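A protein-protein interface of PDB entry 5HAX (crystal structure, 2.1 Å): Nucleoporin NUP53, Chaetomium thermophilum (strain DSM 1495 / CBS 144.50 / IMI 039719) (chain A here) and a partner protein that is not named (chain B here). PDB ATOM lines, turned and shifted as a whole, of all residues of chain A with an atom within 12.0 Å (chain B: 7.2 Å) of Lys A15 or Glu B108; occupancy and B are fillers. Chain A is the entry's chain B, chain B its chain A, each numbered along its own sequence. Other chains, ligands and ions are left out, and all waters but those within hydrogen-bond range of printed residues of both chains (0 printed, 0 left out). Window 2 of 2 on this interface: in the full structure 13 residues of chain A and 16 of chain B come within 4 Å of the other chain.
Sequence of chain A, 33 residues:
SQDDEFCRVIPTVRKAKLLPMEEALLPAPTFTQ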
ATOM      1  N   ARG A  14     -13.976   8.003   3.473  1.00  0.00           N
ATOM      2  CA  ARG A  14     -13.187   8.629   4.528  1.00  0.00           C
ATOM      3  C   ARG A  14     -11.873   9.180   3.978  1.00  0.00           C
ATOM      4  O   ARG A  14     -11.071   8.439   3.408  1.00  0.00           O
ATOM      5  CB  ARG A  14     -12.905   7.625   5.652  1.00  0.00           C
ATOM      6  CG  ARG A  14     -14.141   7.185   6.428  1.00  0.00           C
ATOM      7  CD  ARG A  14     -13.787   6.220   7.558  1.00  0.00           C
ATOM      8  NE  ARG A  14     -14.973   5.748   8.272  1.00  0.00           N
ATOM      9  CZ  ARG A  14     -14.957   4.826   9.231  1.00  0.00           C
ATOM     10  NH1 ARG A  14     -16.089   4.464   9.822  1.00  0.00           N
ATOM     11  NH2 ARG A  14     -13.814   4.262   9.603  1.00  0.00           N
ATOM     12  N   LYS A  15     -11.666  10.486   4.146  1.00  0.00           N
ATOM     13  CA  LYS A  15     -10.411  11.106   3.739  1.00  0.00           C
ATOM     14  C   LYS A  15      -9.243  10.469   4.480  1.00  0.00           C
ATOM     15  O   LYS A  15      -9.240  10.394   5.712  1.00  0.00           O
ATOM     16  CB  LYS A  15     -10.449  12.612   4.009  1.00  0.00           C
ATOM     17  CG  LYS A  15     -11.058  13.446   2.889  1.00  0.00           C
ATOM     18  CD  LYS A  15     -10.894  14.934   3.174  1.00  0.00           C
ATOM     19  CE  LYS A  15     -11.142  15.784   1.936  1.00  0.00           C
ATOM     20  NZ  LYS A  15     -12.573  15.800   1.526  1.00  0.00           N
ATOM     21  N   ALA A  16      -8.249  10.012   3.721  1.00  0.00           N
ATOM     22  CA  ALA A  16      -7.105   9.331   4.310  1.00  0.00           C
ATOM     23  C   ALA A  16      -6.336  10.260   5.242  1.00  0.00           C
ATOM     24  O   ALA A  16      -6.035  11.406   4.892  1.00  0.00           O
ATOM     25  CB  ALA A  16      -6.181   8.810   3.209  1.00  0.00           C
ATOM     26  N   LYS A  17      -6.021   9.757   6.433  1.00  0.00           N
ATOM     27  CA  LYS A  17      -5.206  10.495   7.389  1.00  0.00           C
ATOM     28  C   LYS A  17      -3.781  10.610   6.860  1.00  0.00           C
ATOM     29  O   LYS A  17      -3.117   9.594   6.627  1.00  0.00           O
ATOM     30  CB  LYS A  17      -5.225   9.783   8.740  1.00  0.00           C
ATOM     31  CG  LYS A  17      -4.376  10.423   9.833  1.00  0.00           C
ATOM     32  CD  LYS A  17      -3.816   9.351  10.758  1.00  0.00           C
ATOM     33  CE  LYS A  17      -3.550   9.881  12.156  1.00  0.00           C
ATOM     34  NZ  LYS A  17      -3.141   8.784  13.077  1.00  0.00           N
ATOM     35  N   LEU A  18      -3.310  11.843   6.673  1.00  0.00           N
ATOM     36  CA  LEU A  18      -1.962  12.108   6.171  1.00  0.00           C
ATOM     37  C   LEU A  18      -1.064  12.420   7.365  1.00  0.00           C
ATOM     38  O   LEU A  18      -1.104  13.523   7.915  1.00  0.00           O
ATOM     39  CB  LEU A  18      -1.969  13.255   5.167  1.00  0.00           C
ATOM     40  CG  LEU A  18      -2.956  13.154   4.003  1.00  0.00           C
ATOM     41  CD1 LEU A  18      -2.977  14.465   3.235  1.00  0.00           C
ATOM     42  CD2 LEU A  18      -2.608  11.997   3.076  1.00  0.00           C
ATOM     43  N   LEU A  19      -0.254  11.442   7.762  1.00  0.00           N
ATOM     44  CA  LEU A  19       0.671  11.631   8.866  1.00  0.00           C
ATOM     45  C   LEU A  19       1.723  12.678   8.500  1.00  0.00           C
ATOM     46  O   LEU A  19       1.976  12.931   7.319  1.00  0.00           O
ATOM     47  CB  LEU A  19       1.327  10.301   9.228  1.00  0.00           C
ATOM     48  CG  LEU A  19       0.372   9.222   9.744  1.00  0.00           C
ATOM     49  CD1 LEU A  19       1.106   7.901   9.906  1.00  0.00           C
ATOM     50  CD2 LEU A  19      -0.270   9.640  11.059  1.00  0.00           C
ATOM     51  N   HIS B  65     -18.741   7.062  -7.582  1.00  0.00           N
ATOM     52  CA  HIS B  65     -17.912   8.225  -7.881  1.00  0.00           C
ATOM     53  C   HIS B  65     -17.668   8.362  -9.380  1.00  0.00           C
ATOM     54  O   HIS B  65     -17.698   9.474  -9.919  1.00  0.00           O
ATOM     55  CB  HIS B  65     -16.581   8.127  -7.136  1.00  0.00           C
ATOM     56  CG  HIS B  65     -16.695   8.323  -5.655  1.00  0.00           C
ATOM     57  ND1 HIS B  65     -17.178   9.485  -5.092  1.00  0.00           N
ATOM     58  CD2 HIS B  65     -16.370   7.511  -4.621  1.00  0.00           C
ATOM     59  CE1 HIS B  65     -17.154   9.376  -3.775  1.00  0.00           C
ATOM     60  NE2 HIS B  65     -16.668   8.188  -3.464  1.00  0.00           N
ATOM     61  N   SER B  90     -10.773  16.057  -9.513  1.00  0.00           N
ATOM     62  CA  SER B  90      -9.681  16.416  -8.616  1.00  0.00           C
ATOM     63  C   SER B  90      -9.558  15.475  -7.420  1.00  0.00           C
ATOM     64  O   SER B  90      -8.858  15.807  -6.457  1.00  0.00           O
ATOM     65  CB  SER B  90      -9.865  17.852  -8.118  1.00  0.00           C
ATOM     66  OG  SER B  90     -11.096  18.003  -7.433  1.00  0.00           O
ATOM     67  N   SER B  91     -10.209  14.312  -7.458  1.00  0.00           N
ATOM     68  CA  SER B  91     -10.221  13.380  -6.339  1.00  0.00           C
ATOM     69  C   SER B  91      -9.617  12.044  -6.753  1.00  0.00           C
ATOM     70  O   SER B  91      -9.767  11.605  -7.896  1.00  0.00           O
ATOM     71  CB  SER B  91     -11.648  13.170  -5.816  1.00  0.00           C
ATOM     72  OG  SER B  91     -12.151  14.355  -5.223  1.00  0.00           O
ATOM     73  N   LEU B  92      -8.938  11.397  -5.803  1.00  0.00           N
ATOM     74  CA  LEU B  92      -8.239  10.139  -6.037  1.00  0.00           C
ATOM     75  C   LEU B  92      -8.637   9.117  -4.982  1.00  0.00           C
ATOM     76  O   LEU B  92      -8.747   9.448  -3.798  1.00  0.00           O
ATOM     77  CB  LEU B  92      -6.721  10.346  -6.007  1.00  0.00           C
ATOM     78  CG  LEU B  92      -5.867   9.086  -6.141  1.00  0.00           C
ATOM     79  CD1 LEU B  92      -6.133   8.388  -7.469  1.00  0.00           C
ATOM     80  CD2 LEU B  92      -4.400   9.439  -5.996  1.00  0.00           C
ATOM     81  N   PHE B  93      -8.827   7.869  -5.413  1.00  0.00           N
ATOM     82  CA  PHE B  93      -9.252   6.790  -4.523  1.00  0.00           C
ATOM     83  C   PHE B  93      -8.436   5.538  -4.811  1.00  0.00           C
ATOM     84  O   PHE B  93      -8.421   5.054  -5.947  1.00  0.00           O
ATOM     85  CB  PHE B  93     -10.747   6.504  -4.689  1.00  0.00           C
ATOM     86  CG  PHE B  93     -11.622   7.672  -4.347  1.00  0.00           C
ATOM     87  CD1 PHE B  93     -11.974   7.927  -3.033  1.00  0.00           C
ATOM     88  CD2 PHE B  93     -12.087   8.521  -5.338  1.00  0.00           C
ATOM     89  CE1 PHE B  93     -12.777   9.006  -2.712  1.00  0.00           C
ATOM     90  CE2 PHE B  93     -12.891   9.601  -5.025  1.00  0.00           C
ATOM     91  CZ  PHE B  93     -13.236   9.843  -3.709  1.00  0.00           C
ATOM     92  N   LEU B 104     -11.998   2.311   0.812  1.00  0.00           N
ATOM     93  CA  LEU B 104     -11.406   3.233  -0.150  1.00  0.00           C
ATOM     94  C   LEU B 104     -10.525   4.243   0.576  1.00  0.00           C
ATOM     95  O   LEU B 104     -10.993   4.956   1.470  1.00  0.00           O
ATOM     96  CB  LEU B 104     -12.493   3.949  -0.949  1.00  0.00           C
ATOM     97  CG  LEU B 104     -13.410   3.069  -1.802  1.00  0.00           C
ATOM     98  CD1 LEU B 104     -14.440   3.931  -2.514  1.00  0.00           C
ATOM     99  CD2 LEU B 104     -12.615   2.249  -2.808  1.00  0.00           C
ATOM    100  N   ILE B 105      -9.251   4.298   0.189  1.00  0.00           N
ATOM    101  CA  ILE B 105      -8.321   5.314   0.677  1.00  0.00           C
ATOM    102  C   ILE B 105      -8.528   6.553  -0.191  1.00  0.00           C
ATOM    103  O   ILE B 105      -8.075   6.604  -1.335  1.00  0.00           O
ATOM    104  CB  ILE B 105      -6.869   4.830   0.632  1.00  0.00           C
ATOM    105  CG1 ILE B 105      -6.710   3.558   1.472  1.00  0.00           C
ATOM    106  CG2 ILE B 105      -5.926   5.921   1.125  1.00  0.00           C
ATOM    107  CD1 ILE B 105      -5.354   2.899   1.336  1.00  0.00           C
ATOM    108  N   GLY B 106      -9.213   7.557   0.352  1.00  0.00           N
ATOM    109  CA  GLY B 106      -9.519   8.764  -0.399  1.00  0.00           C
ATOM    110  C   GLY B 106      -8.482   9.854  -0.172  1.00  0.00           C
ATOM    111  O   GLY B 106      -7.990  10.043   0.938  1.00  0.00           O
ATOM    112  N   TYR B 107      -8.157  10.567  -1.249  1.00  0.00           N
ATOM    113  CA  TYR B 107      -7.262  11.720  -1.193  1.00  0.00           C
ATOM    114  C   TYR B 107      -7.834  12.791  -2.110  1.00  0.00           C
ATOM    115  O   TYR B 107      -7.846  12.620  -3.334  1.00  0.00           O
ATOM    116  CB  TYR B 107      -5.838  11.352  -1.607  1.00  0.00           C
ATOM    117  CG  TYR B 107      -4.933  12.553  -1.751  1.00  0.00           C
ATOM    118  CD1 TYR B 107      -4.688  13.117  -2.995  1.00  0.00           C
ATOM    119  CD2 TYR B 107      -4.335  13.133  -0.640  1.00  0.00           C
ATOM    120  CE1 TYR B 107      -3.865  14.219  -3.130  1.00  0.00           C
ATOM    121  CE2 TYR B 107      -3.512  14.235  -0.765  1.00  0.00           C
ATOM    122  CZ  TYR B 107      -3.280  14.773  -2.013  1.00  0.00           C
ATOM    123  OH  TYR B 107      -2.460  15.872  -2.146  1.00  0.00           O
ATOM    124  N   GLU B 108      -8.296  13.897  -1.518  1.00  0.00           N
ATOM    125  CA  GLU B 108      -9.028  14.924  -2.250  1.00  0.00           C
ATOM    126  C   GLU B 108      -8.458  16.317  -2.002  1.00  0.00           C
ATOM    127  O   GLU B 108      -9.159  17.312  -2.212  1.00  0.00           O
ATOM    128  CB  GLU B 108     -10.511  14.879  -1.879  1.00  0.00           C
ATOM    129  CG  GLU B 108     -11.054  13.458  -1.774  1.00  0.00           C
ATOM    130  CD  GLU B 108     -12.563  13.405  -1.625  1.00  0.00           C
ATOM    131  OE1 GLU B 108     -13.248  14.327  -2.117  1.00  0.00           O
ATOM    132  OE2 GLU B 108     -13.064  12.438  -1.014  1.00  0.00           O
ATOM    133  N   GLU B 109      -7.199  16.411  -1.569  1.00  0.00           N
ATOM    134  CA  GLU B 109      -6.584  17.717  -1.358  1.00  0.00           C
ATOM    135  C   GLU B 109      -6.415  18.474  -2.668  1.00  0.00           C
ATOM    136  O   GLU B 109      -6.455  19.709  -2.676  1.00  0.00           O
ATOM    137  CB  GLU B 109      -5.221  17.561  -0.679  1.00  0.00           C
ATOM    138  CG  GLU B 109      -5.251  16.809   0.640  1.00  0.00           C
ATOM    139  CD  GLU B 109      -6.197  17.431   1.646  1.00  0.00           C
ATOM    140  OE1 GLU B 109      -7.223  16.796   1.970  1.00  0.00           O
ATOM    141  OE2 GLU B 109      -5.914  18.555   2.114  1.00  0.00           O
ATOM    142  N   ALA B 110      -6.223  17.757  -3.773  1.00  0.00           N
ATOM    143  CA  ALA B 110      -5.934  18.396  -5.048  1.00  0.00           C
ATOM    144  C   ALA B 110      -7.049  19.355  -5.445  1.00  0.00           C
ATOM    145  O   ALA B 110      -8.233  19.120  -5.184  1.00  0.00           O
ATOM    146  CB  ALA B 110      -5.739  17.346  -6.141  1.00  0.00           C
ATOM    147  N   THR B 111      -6.649  20.444  -6.096  1.00  0.00           N
ATOM    148  CA  THR B 111      -7.564  21.501  -6.504  1.00  0.00           C
ATOM    149  C   THR B 111      -7.984  21.403  -7.963  1.00  0.00           C
ATOM    150  O   THR B 111      -9.072  21.874  -8.310  1.00  0.00           O
ATOM    151  CB  THR B 111      -6.927  22.877  -6.252  1.00  0.00           C
ATOM    152  OG1 THR B 111      -7.731  23.898  -6.856  1.00  0.00           O
ATOM    153  CG2 THR B 111      -5.506  22.950  -6.819  1.00  0.00           C
ATOM    154  N   ILE B 114      -6.910  15.648 -11.950  1.00  0.00           N
ATOM    155  CA  ILE B 114      -5.776  14.729 -11.959  1.00  0.00           C
ATOM    156  C   ILE B 114      -5.627  14.147 -13.358  1.00  0.00           C
ATOM    157  O   ILE B 114      -6.598  13.652 -13.943  1.00  0.00           O
ATOM    158  CB  ILE B 114      -5.969  13.617 -10.913  1.00  0.00           C
ATOM    159  CG1 ILE B 114      -5.897  14.204  -9.500  1.00  0.00           C
ATOM    160  CG2 ILE B 114      -4.910  12.525 -11.075  1.00  0.00           C
ATOM    161  CD1 ILE B 114      -6.376  13.256  -8.420  1.00  0.00           C
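The backbone carbonyl oxygen (O) of Gly B106 lies within hydrogen-bond range of the backbone NH (N) of Ala A16 (2.8 Å).
The side-chain carboxylate (OE1) of Glu B108 lies within salt-bridge range of the side-chain amino group (NZ) of Lys A15 (3.99 Å).
The side-chain hydroxyl (OG) of Ser B91 is in hydrogen-bond range of the side-chain carboxylate (OE1) of Glu B108.
Among the printed residues, merely in contact across the chains: Ala A16 with Ile B105, Arg A14 with Gly B106, Lys A15 with Gly B106 and Arg A14 with Leu B104.
Of chain B, only Gly B106 (3.8 Å) and Glu B108 (3.96 Å) come within 4 Å of Lys A15.
Glu B108 touches just one residue of chain A: Lys A15 (3.96 Å).
No residue of chain A comes within 4 Å of Ser B90.
No residue of chain A comes within 4 Å of Ser B91.
Gly B106 touches just these residues of chain A: Arg A14, Lys A15 and Ala A16.
No residue of chain A comes within 4 Å of Tyr B107.
Glu B109 touches none of the printed residues of chain A.
Ala B110 touches none of the printed residues of chain A.
Printed residues of chain A within 4 Å of Ile B105: Ala A16.
Printed residues of chain B within 4 Å of Ala A16: Ile B105 (3.6 Å) and Gly B106 (2.8 Å).
Of the printed residues of chain A, Leu B104 touches Arg A14.
Printed residues of chain B within 4 Å of Arg A14: Leu B104 and Gly B106.
The nearest residue of chain B that does not touch Lys A15 is Glu B109 (4.05 Å).
The nearest residue of chain A that does not touch Glu B108 is Arg A14 (6.1 Å).
The nearest printed residue of chain B that does not touch Arg A14 is Ile B105 (4.8 Å).
Printed residues of chain B that touch a printed residue of chain A: Leu B104, Ile B105, Gly B106 and Glu B108.
Printed residues of chain A that touch a printed residue of chain B: Arg A14, Lys A15 and Ala A16.
Hydrophobic or aromatic side chains of chain A within 4 Å of the printed part of chain B: Ala A16.
Among the printed residues, Asp or Glu carboxylates within 4 Å of a Lys or Arg side-chain nitrogen of the other chain: Lys A15 with Glu B108.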
